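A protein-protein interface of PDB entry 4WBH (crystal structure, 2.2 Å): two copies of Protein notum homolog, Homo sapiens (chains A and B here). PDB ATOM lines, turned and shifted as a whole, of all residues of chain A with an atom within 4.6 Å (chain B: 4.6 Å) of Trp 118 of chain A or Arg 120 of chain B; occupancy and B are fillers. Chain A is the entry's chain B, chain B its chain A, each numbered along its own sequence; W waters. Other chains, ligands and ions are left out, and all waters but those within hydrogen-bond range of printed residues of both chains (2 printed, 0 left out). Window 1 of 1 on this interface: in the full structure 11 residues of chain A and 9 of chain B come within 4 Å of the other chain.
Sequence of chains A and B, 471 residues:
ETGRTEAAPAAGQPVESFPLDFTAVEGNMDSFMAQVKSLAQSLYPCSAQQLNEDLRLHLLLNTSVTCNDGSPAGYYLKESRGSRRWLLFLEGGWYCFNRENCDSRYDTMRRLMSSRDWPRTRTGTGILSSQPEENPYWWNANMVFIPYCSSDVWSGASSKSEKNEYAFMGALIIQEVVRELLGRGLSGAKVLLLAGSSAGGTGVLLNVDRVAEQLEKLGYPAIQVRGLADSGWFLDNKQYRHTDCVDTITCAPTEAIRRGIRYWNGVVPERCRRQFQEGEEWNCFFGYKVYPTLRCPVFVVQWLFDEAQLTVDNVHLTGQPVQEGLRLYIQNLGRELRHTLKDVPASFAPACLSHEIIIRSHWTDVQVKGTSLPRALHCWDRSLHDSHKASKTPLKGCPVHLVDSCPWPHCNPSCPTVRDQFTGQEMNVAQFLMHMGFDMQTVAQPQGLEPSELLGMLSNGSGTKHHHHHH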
ATOM      1  N   LEU A  57      10.123  -5.572  29.734  1.00  0.00           N
ATOM      2  CA  LEU A  57       9.177  -6.676  29.617  1.00  0.00           C
ATOM      3  C   LEU A  57       9.577  -7.710  28.571  1.00  0.00           C
ATOM      4  O   LEU A  57       9.999  -7.373  27.481  1.00  0.00           O
ATOM      5  CB  LEU A  57       7.771  -6.144  29.333  1.00  0.00           C
ATOM      6  CG  LEU A  57       6.622  -7.130  29.086  1.00  0.00           C
ATOM      7  CD1 LEU A  57       6.402  -8.043  30.289  1.00  0.00           C
ATOM      8  CD2 LEU A  57       5.356  -6.356  28.767  1.00  0.00           C
ATOM      9  N   LEU A  59       7.562 -11.178  27.233  1.00  0.00           N
ATOM     10  CA  LEU A  59       6.441 -12.099  27.348  1.00  0.00           C
ATOM     11  C   LEU A  59       6.955 -13.492  27.011  1.00  0.00           C
ATOM     12  O   LEU A  59       7.795 -13.640  26.122  1.00  0.00           O
ATOM     13  CB  LEU A  59       5.300 -11.698  26.405  1.00  0.00           C
ATOM     14  CG  LEU A  59       4.618 -10.329  26.587  1.00  0.00           C
ATOM     15  CD1 LEU A  59       3.757  -9.997  25.380  1.00  0.00           C
ATOM     16  CD2 LEU A  59       3.791 -10.247  27.867  1.00  0.00           C
ATOM     17  N   CYS A  67      -1.609 -16.192  31.603  1.00  0.00           N
ATOM     18  CA  CYS A  67      -2.404 -15.559  32.653  1.00  0.00           C
ATOM     19  C   CYS A  67      -3.823 -16.131  32.659  1.00  0.00           C
ATOM     20  O   CYS A  67      -4.163 -16.933  31.796  1.00  0.00           O
ATOM     21  CB  CYS A  67      -2.439 -14.044  32.435  1.00  0.00           C
ATOM     22  SG  CYS A  67      -0.798 -13.291  32.450  1.00  0.00           S
ATOM     23  N   SER A  71      -4.138 -14.491  27.974  1.00  0.00           N
ATOM     24  CA  SER A  71      -3.057 -13.610  27.527  1.00  0.00           C
ATOM     25  C   SER A  71      -1.712 -14.197  27.946  1.00  0.00           C
ATOM     26  O   SER A  71      -1.655 -14.933  28.922  1.00  0.00           O
ATOM     27  CB  SER A  71      -3.232 -12.218  28.119  1.00  0.00           C
ATOM     28  OG  SER A  71      -3.208 -12.264  29.536  1.00  0.00           O
ATOM     29  N   PRO A  72      -0.629 -13.893  27.201  1.00  0.00           N
ATOM     30  CA  PRO A  72       0.667 -14.465  27.561  1.00  0.00           C
ATOM     31  C   PRO A  72       1.197 -13.926  28.883  1.00  0.00           C
ATOM     32  O   PRO A  72       1.075 -12.736  29.167  1.00  0.00           O
ATOM     33  CB  PRO A  72       1.591 -13.999  26.426  1.00  0.00           C
ATOM     34  CG  PRO A  72       0.923 -12.783  25.862  1.00  0.00           C
ATOM     35  CD  PRO A  72      -0.546 -13.074  25.975  1.00  0.00           C
ATOM     36  N   ALA A  73       1.790 -14.811  29.676  1.00  0.00           N
ATOM     37  CA  ALA A  73       2.478 -14.419  30.895  1.00  0.00           C
ATOM     38  C   ALA A  73       3.838 -13.840  30.504  1.00  0.00           C
ATOM     39  O   ALA A  73       4.139 -13.705  29.317  1.00  0.00           O
ATOM     40  CB  ALA A  73       2.642 -15.624  31.806  1.00  0.00           C
ATOM     41  N   GLY A  74       4.660 -13.508  31.491  1.00  0.00           N
ATOM     42  CA  GLY A  74       5.979 -12.990  31.205  1.00  0.00           C
ATOM     43  C   GLY A  74       6.673 -12.429  32.421  1.00  0.00           C
ATOM     44  O   GLY A  74       6.292 -12.718  33.562  1.00  0.00           O
ATOM     45  N   TYR A  76       9.674  -9.061  33.693  1.00  0.00           N
ATOM     46  CA  TYR A  76      10.531  -7.914  33.398  1.00  0.00           C
ATOM     47  C   TYR A  76      11.951  -8.254  33.824  1.00  0.00           C
ATOM     48  O   TYR A  76      12.149  -8.930  34.828  1.00  0.00           O
ATOM     49  CB  TYR A  76      10.065  -6.690  34.173  1.00  0.00           C
ATOM     50  CG  TYR A  76       8.703  -6.159  33.782  1.00  0.00           C
ATOM     51  CD1 TYR A  76       7.541  -6.786  34.225  1.00  0.00           C
ATOM     52  CD2 TYR A  76       8.578  -4.993  33.009  1.00  0.00           C
ATOM     53  CE1 TYR A  76       6.291  -6.300  33.883  1.00  0.00           C
ATOM     54  CE2 TYR A  76       7.328  -4.489  32.665  1.00  0.00           C
ATOM     55  CZ  TYR A  76       6.189  -5.149  33.106  1.00  0.00           C
ATOM     56  OH  TYR A  76       4.947  -4.686  32.794  1.00  0.00           O
ATOM     57  N   ARG A 111      -6.147  -6.179  35.996  1.00  0.00           N
ATOM     58  CA  ARG A 111      -4.676  -6.181  35.990  1.00  0.00           C
ATOM     59  C   ARG A 111      -4.095  -7.479  36.557  1.00  0.00           C
ATOM     60  O   ARG A 111      -3.009  -7.896  36.161  1.00  0.00           O
ATOM     61  CB  ARG A 111      -4.097  -4.972  36.752  1.00  0.00           C
ATOM     62  CG  ARG A 111      -2.588  -5.090  37.044  1.00  0.00           C
ATOM     63  CD  ARG A 111      -1.997  -3.975  37.912  1.00  0.00           C
ATOM     64  NE  ARG A 111      -2.629  -3.886  39.230  1.00  0.00           N
ATOM     65  CZ  ARG A 111      -2.173  -4.460  40.345  1.00  0.00           C
ATOM     66  NH1 ARG A 111      -1.057  -5.178  40.341  1.00  0.00           N
ATOM     67  NH2 ARG A 111      -2.847  -4.309  41.479  1.00  0.00           N
ATOM     68  N   SER A 114      -4.602 -10.682  33.802  1.00  0.00           N
ATOM     69  CA  SER A 114      -4.274 -10.424  32.405  1.00  0.00           C
ATOM     70  C   SER A 114      -2.894  -9.776  32.291  1.00  0.00           C
ATOM     71  O   SER A 114      -2.412  -9.170  33.246  1.00  0.00           O
ATOM     72  CB  SER A 114      -5.339  -9.487  31.807  1.00  0.00           C
ATOM     73  OG  SER A 114      -5.237  -9.403  30.398  1.00  0.00           O
ATOM     74  N   SER A 115      -2.266  -9.896  31.126  1.00  0.00           N
ATOM     75  CA  SER A 115      -1.033  -9.151  30.836  1.00  0.00           C
ATOM     76  C   SER A 115      -1.315  -7.971  29.896  1.00  0.00           C
ATOM     77  O   SER A 115      -0.395  -7.267  29.460  1.00  0.00           O
ATOM     78  CB  SER A 115       0.010 -10.071  30.202  1.00  0.00           C
ATOM     79  OG  SER A 115      -0.455 -10.533  28.947  1.00  0.00           O
ATOM     80  N   ARG A 116      -2.592  -7.764  29.596  1.00  0.00           N
ATOM     81  CA  ARG A 116      -3.013  -6.804  28.564  1.00  0.00           C
ATOM     82  C   ARG A 116      -2.683  -5.350  28.929  1.00  0.00           C
ATOM     83  O   ARG A 116      -2.420  -4.530  28.060  1.00  0.00           O
ATOM     84  CB  ARG A 116      -4.508  -6.959  28.254  1.00  0.00           C
ATOM     85  CG  ARG A 116      -4.855  -8.260  27.537  1.00  0.00           C
ATOM     86  CD  ARG A 116      -6.361  -8.543  27.539  1.00  0.00           C
ATOM     87  NE  ARG A 116      -7.085  -7.740  26.548  1.00  0.00           N
ATOM     88  CZ  ARG A 116      -8.416  -7.652  26.462  1.00  0.00           C
ATOM     89  NH1 ARG A 116      -9.197  -8.310  27.323  1.00  0.00           N
ATOM     90  NH2 ARG A 116      -8.969  -6.890  25.511  1.00  0.00           N
ATOM     91  N   ASP A 117      -2.689  -5.045  30.218  1.00  0.00           N
ATOM     92  CA  ASP A 117      -2.433  -3.686  30.641  1.00  0.00           C
ATOM     93  C   ASP A 117      -1.024  -3.451  31.184  1.00  0.00           C
ATOM     94  O   ASP A 117      -0.747  -2.363  31.686  1.00  0.00           O
ATOM     95  CB  ASP A 117      -3.495  -3.222  31.645  1.00  0.00           C
ATOM     96  CG  ASP A 117      -4.877  -3.056  31.006  1.00  0.00           C
ATOM     97  OD1 ASP A 117      -4.968  -2.515  29.878  1.00  0.00           O
ATOM     98  OD2 ASP A 117      -5.876  -3.458  31.637  1.00  0.00           O
ATOM     99  N   TRP A 118      -0.133  -4.440  31.056  1.00  0.00           N
ATOM    100  CA  TRP A 118       1.234  -4.283  31.580  1.00  0.00           C
ATOM    101  C   TRP A 118       2.005  -3.254  30.756  1.00  0.00           C
ATOM    102  O   TRP A 118       1.925  -3.268  29.526  1.00  0.00           O
ATOM    103  CB  TRP A 118       2.052  -5.589  31.566  1.00  0.00           C
ATOM    104  CG  TRP A 118       1.577  -6.737  32.419  1.00  0.00           C
ATOM    105  CD1 TRP A 118       0.617  -6.717  33.396  1.00  0.00           C
ATOM    106  CD2 TRP A 118       2.085  -8.085  32.384  1.00  0.00           C
ATOM    107  NE1 TRP A 118       0.474  -7.976  33.939  1.00  0.00           N
ATOM    108  CE2 TRP A 118       1.374  -8.826  33.342  1.00  0.00           C
ATOM    109  CE3 TRP A 118       3.062  -8.732  31.617  1.00  0.00           C
ATOM    110  CZ2 TRP A 118       1.602 -10.194  33.554  1.00  0.00           C
ATOM    111  CZ3 TRP A 118       3.288 -10.090  31.826  1.00  0.00           C
ATOM    112  CH2 TRP A 118       2.557 -10.804  32.782  1.00  0.00           C
ATOM    113  N   PRO A 119       2.777  -2.379  31.428  1.00  0.00           N
ATOM    114  CA  PRO A 119       3.673  -1.474  30.728  1.00  0.00           C
ATOM    115  C   PRO A 119       4.884  -2.206  30.153  1.00  0.00           C
ATOM    116  O   PRO A 119       5.231  -3.286  30.622  1.00  0.00           O
ATOM    117  CB  PRO A 119       4.114  -0.497  31.822  1.00  0.00           C
ATOM    118  CG  PRO A 119       3.126  -0.672  32.922  1.00  0.00           C
ATOM    119  CD  PRO A 119       2.759  -2.112  32.871  1.00  0.00           C
ATOM    120  N   ARG A 120       5.515  -1.611  29.143  1.00  0.00           N
ATOM    121  CA  ARG A 120       6.695  -2.185  28.497  1.00  0.00           C
ATOM    122  C   ARG A 120       7.942  -2.202  29.399  1.00  0.00           C
ATOM    123  O   ARG A 120       8.852  -3.017  29.217  1.00  0.00           O
ATOM    124  CB  ARG A 120       6.982  -1.417  27.201  1.00  0.00           C
ATOM    125  CG  ARG A 120       6.050  -1.773  26.042  1.00  0.00           C
ATOM    126  CD  ARG A 120       6.680  -2.818  25.143  1.00  0.00           C
ATOM    127  NE  ARG A 120       5.763  -3.916  24.859  1.00  0.00           N
ATOM    128  CZ  ARG A 120       6.130  -5.194  24.777  1.00  0.00           C
ATOM    129  NH1 ARG A 120       5.221  -6.129  24.521  1.00  0.00           N
ATOM    130  NH2 ARG A 120       7.406  -5.544  24.967  1.00  0.00           N
ATOM    131  N   PRO A 147       5.124 -10.630  37.228  1.00  0.00           N
ATOM    132  CA  PRO A 147       3.821 -10.167  37.669  1.00  0.00           C
ATOM    133  C   PRO A 147       2.857 -11.319  37.937  1.00  0.00           C
ATOM    134  O   PRO A 147       2.982 -12.416  37.361  1.00  0.00           O
ATOM    135  CB  PRO A 147       3.326  -9.306  36.505  1.00  0.00           C
ATOM    136  CG  PRO A 147       4.554  -8.940  35.762  1.00  0.00           C
ATOM    137  CD  PRO A 147       5.462 -10.135  35.892  1.00  0.00           C
ATOM    138  N   CYS A 149      -0.462 -12.882  37.557  1.00  0.00           N
ATOM    139  CA  CYS A 149      -1.671 -12.867  36.724  1.00  0.00           C
ATOM    140  C   CYS A 149      -2.467 -14.175  36.772  1.00  0.00           C
ATOM    141  O   CYS A 149      -3.358 -14.403  35.949  1.00  0.00           O
ATOM    142  CB  CYS A 149      -1.346 -12.468  35.276  1.00  0.00           C
ATOM    143  SG  CYS A 149      -0.200 -13.549  34.381  1.00  0.00           S
ATOM    144  N   LEU B  55      -5.100  -3.291  19.919  1.00  0.00           N
ATOM    145  CA  LEU B  55      -3.999  -2.510  19.356  1.00  0.00           C
ATOM    146  C   LEU B  55      -2.764  -2.755  20.233  1.00  0.00           C
ATOM    147  O   LEU B  55      -2.894  -2.763  21.453  1.00  0.00           O
ATOM    148  CB  LEU B  55      -4.360  -1.025  19.308  1.00  0.00           C
ATOM    149  CG  LEU B  55      -5.332  -0.503  18.229  1.00  0.00           C
ATOM    150  CD1 LEU B  55      -6.751  -1.042  18.396  1.00  0.00           C
ATOM    151  CD2 LEU B  55      -5.352   1.025  18.227  1.00  0.00           C
ATOM    152  N   ARG B  56      -1.598  -3.000  19.624  1.00  0.00           N
ATOM    153  CA  ARG B  56      -0.359  -3.262  20.396  1.00  0.00           C
ATOM    154  C   ARG B  56       0.568  -2.067  20.403  1.00  0.00           C
ATOM    155  O   ARG B  56       0.765  -1.433  19.371  1.00  0.00           O
ATOM    156  CB  ARG B  56       0.424  -4.456  19.837  1.00  0.00           C
ATOM    157  CG  ARG B  56      -0.337  -5.779  19.801  1.00  0.00           C
ATOM    158  CD  ARG B  56       0.397  -6.817  18.953  1.00  0.00           C
ATOM    159  NE  ARG B  56       1.803  -6.934  19.346  1.00  0.00           N
ATOM    160  CZ  ARG B  56       2.845  -6.714  18.545  1.00  0.00           C
ATOM    161  NH1 ARG B  56       4.078  -6.852  19.027  1.00  0.00           N
ATOM    162  NH2 ARG B  56       2.669  -6.381  17.267  1.00  0.00           N
ATOM    163  N   LEU B  57       1.180  -1.808  21.555  1.00  0.00           N
ATOM    164  CA  LEU B  57       2.036  -0.646  21.730  1.00  0.00           C
ATOM    165  C   LEU B  57       3.398  -0.815  21.080  1.00  0.00           C
ATOM    166  O   LEU B  57       4.076  -1.828  21.287  1.00  0.00           O
ATOM    167  CB  LEU B  57       2.204  -0.309  23.219  1.00  0.00           C
ATOM    168  CG  LEU B  57       3.187   0.824  23.553  1.00  0.00           C
ATOM    169  CD1 LEU B  57       2.713   2.191  23.059  1.00  0.00           C
ATOM    170  CD2 LEU B  57       3.501   0.871  25.046  1.00  0.00           C
ATOM    171  N   TYR B  76      -0.015   2.898  19.135  1.00  0.00           N
ATOM    172  CA  TYR B  76      -0.612   1.578  19.247  1.00  0.00           C
ATOM    173  C   TYR B  76      -1.085   1.230  17.851  1.00  0.00           C
ATOM    174  O   TYR B  76      -1.615   2.102  17.147  1.00  0.00           O
ATOM    175  CB  TYR B  76      -1.819   1.607  20.181  1.00  0.00           C
ATOM    176  CG  TYR B  76      -1.524   1.794  21.658  1.00  0.00           C
ATOM    177  CD1 TYR B  76      -1.427   3.072  22.220  1.00  0.00           C
ATOM    178  CD2 TYR B  76      -1.370   0.689  22.499  1.00  0.00           C
ATOM    179  CE1 TYR B  76      -1.173   3.236  23.579  1.00  0.00           C
ATOM    180  CE2 TYR B  76      -1.124   0.847  23.856  1.00  0.00           C
ATOM    181  CZ  TYR B  76      -1.022   2.112  24.386  1.00  0.00           C
ATOM    182  OH  TYR B  76      -0.774   2.255  25.726  1.00  0.00           O
ATOM    183  N   TRP B 118       2.152   3.355  30.316  1.00  0.00           N
ATOM    184  CA  TRP B 118       1.290   2.977  29.184  1.00  0.00           C
ATOM    185  C   TRP B 118       1.117   1.464  29.050  1.00  0.00           C
ATOM    186  O   TRP B 118       2.099   0.712  28.989  1.00  0.00           O
ATOM    187  CB  TRP B 118       1.843   3.474  27.859  1.00  0.00           C
ATOM    188  CG  TRP B 118       1.827   4.947  27.629  1.00  0.00           C
ATOM    189  CD1 TRP B 118       1.265   5.919  28.421  1.00  0.00           C
ATOM    190  CD2 TRP B 118       2.387   5.617  26.503  1.00  0.00           C
ATOM    191  NE1 TRP B 118       1.458   7.157  27.851  1.00  0.00           N
ATOM    192  CE2 TRP B 118       2.141   7.000  26.672  1.00  0.00           C
ATOM    193  CE3 TRP B 118       3.069   5.183  25.359  1.00  0.00           C
ATOM    194  CZ2 TRP B 118       2.574   7.955  25.749  1.00  0.00           C
ATOM    195  CZ3 TRP B 118       3.492   6.135  24.434  1.00  0.00           C
ATOM    196  CH2 TRP B 118       3.244   7.506  24.638  1.00  0.00           C
ATOM    197  N   PRO B 119      -0.137   1.009  28.946  1.00  0.00           N
ATOM    198  CA  PRO B 119      -0.327  -0.431  28.824  1.00  0.00           C
ATOM    199  C   PRO B 119       0.219  -0.933  27.493  1.00  0.00           C
ATOM    200  O   PRO B 119       0.336  -0.153  26.552  1.00  0.00           O
ATOM    201  CB  PRO B 119      -1.842  -0.605  28.944  1.00  0.00           C
ATOM    202  CG  PRO B 119      -2.428   0.742  28.653  1.00  0.00           C
ATOM    203  CD  PRO B 119      -1.405   1.750  29.058  1.00  0.00           C
ATOM    204  N   ARG B 120       0.575  -2.216  27.422  1.00  0.00           N
ATOM    205  CA  ARG B 120       1.187  -2.762  26.211  1.00  0.00           C
ATOM    206  C   ARG B 120       0.175  -2.967  25.076  1.00  0.00           C
ATOM    207  O   ARG B 120       0.566  -3.161  23.934  1.00  0.00           O
ATOM    208  CB  ARG B 120       1.947  -4.062  26.509  1.00  0.00           C
ATOM    209  CG  ARG B 120       1.072  -5.275  26.771  1.00  0.00           C
ATOM    210  CD  ARG B 120       1.878  -6.568  26.911  1.00  0.00           C
ATOM    211  NE  ARG B 120       0.965  -7.684  27.160  1.00  0.00           N
ATOM    212  CZ  ARG B 120       0.253  -8.307  26.214  1.00  0.00           C
ATOM    213  NH1 ARG B 120       0.375  -7.976  24.934  1.00  0.00           N
ATOM    214  NH2 ARG B 120      -0.574  -9.284  26.550  1.00  0.00           N
ATOM    215  N   THR B 121      -1.113  -2.943  25.415  1.00  0.00           N
ATOM    216  CA  THR B 121      -2.199  -3.060  24.446  1.00  0.00           C
ATOM    217  C   THR B 121      -3.326  -2.115  24.848  1.00  0.00           C
ATOM    218  O   THR B 121      -3.365  -1.620  25.986  1.00  0.00           O
ATOM    219  CB  THR B 121      -2.827  -4.479  24.368  1.00  0.00           C
ATOM    220  OG1 THR B 121      -3.555  -4.738  25.569  1.00  0.00           O
ATOM    221  CG2 THR B 121      -1.805  -5.594  24.129  1.00  0.00           C
HETATM  222  O   HOH W   1      -5.561  -0.828  28.078  1.00  0.00           O
HETATM  223  O   HOH W   2       4.484   1.082  28.653  1.00  0.00           O
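NE of Arg 120 of chain B is in hydrogen-bond range of O of Ser 115 of chain A, at 2.7 Å. The backbone carbonyl oxygen (O) of Arg 116 of chain A sits at hydrogen-bond distance from the side-chain hydroxyl (OG1) of Thr 121 of chain B (2.7 Å). The backbone carbonyl oxygen (O) of Trp 118 of chain A sits at hydrogen-bond distance from the backbone NH (N) of Arg 120 of chain B.
N of Arg 116 of chain A lies close to OG of Ser 114 of chain A. The backbone NH (N) of Leu 57 of chain A sits at hydrogen-bond distance from the backbone carbonyl oxygen (O) of Arg 120 of chain A, 2.9 Å away. The backbone carbonyl oxygen of Pro 119 of chain A sits at hydrogen-bond distance from the side-chain hydroxyl of Tyr 76 of chain A, 2.6 Å away. The backbone NH (N) of Ser 115 of chain A lies within hydrogen-bond range of the side-chain hydroxyl (OG) of Ser 71 of chain A (3.0 Å). The side-chain sulfur (SG) of Cys 67 of chain A forms a disulfide with the side-chain sulfur (SG) of Cys 149 of chain A. The side-chain hydroxyl of Ser 115 of chain A lies within hydrogen-bond range of the backbone carbonyl oxygen of Pro 72 of chain A (2.7 Å).
Among the printed residues, merely in contact across the chains: Pro 119 of chain A with Trp 118 of chain B, Asp 117 of chain A with Pro 119 of chain B, Trp 118 of chain A with Pro 119 of chain B, Arg 116 of chain A with Arg 120 of chain B, Arg 120 of chain A with Leu 57 of chain B, Pro 72 of chain A with Arg 120 of chain B, Leu 59 of chain A with Arg 120 of chain B and Leu 57 of chain A with Arg 120 of chain B.
Of the printed residues of chain B, Leu 57 of chain A touches Arg 120 (3.9 Å). Printed residues of chain B within 4 Å of Pro 72 of chain A: Arg 120. Of the printed residues of chain B, Asp 117 of chain A touches Pro 119 (3.4 Å). Of the printed residues of chain B, Trp 118 of chain A touches Pro 119 and Arg 120. Of the printed residues of chain B, Pro 119 of chain A touches Trp 118. Arg 120 of chain B touches six residues of chain A. The nearest residue of chain A that does not touch Arg 120 of chain B is Arg 120 of chain A (4.1 Å).
Hydrophobic or aromatic side chains of chain A within 4 Å of the printed part of chain B: Leu 57, Leu 59, Pro 72 and Pro 119. Of the 8 printed residues of chain B, 5 touch a printed residue of chain A. Along chain B the printed residues that touch a printed residue of chain A span positions 57 to 121. Among the printed residues, 11 pairs touch across the chains. Among the printed residues, no Asp or Glu carboxylate lies within 4 Å of a Lys or Arg side-chain nitrogen of the other chain.
Leu 57 of chain A touches Arg 120 of chain B, and with the chains exchanged Arg 120 of chain A touches Leu 57 of chain B. Trp 118 of chain A touches Pro 119 of chain B, and with the chains exchanged Pro 119 of chain A touches Trp 118 of chain B. Trp 118 of chain A touches Arg 120 of chain B, but with the chains exchanged Arg 120 of chain A does not touch Trp 118 of chain B (4.1 Å).
Water W2 lies within hydrogen-bond range of O of Trp 118 of chain B (2.4 Å) and N of Arg 120 of chain A (2.9 Å). Water W1 bridges the side-chain carboxylate (OD1) of Asp 117 of chain A and the backbone carbonyl oxygen (O) of Thr 121 of chain B.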
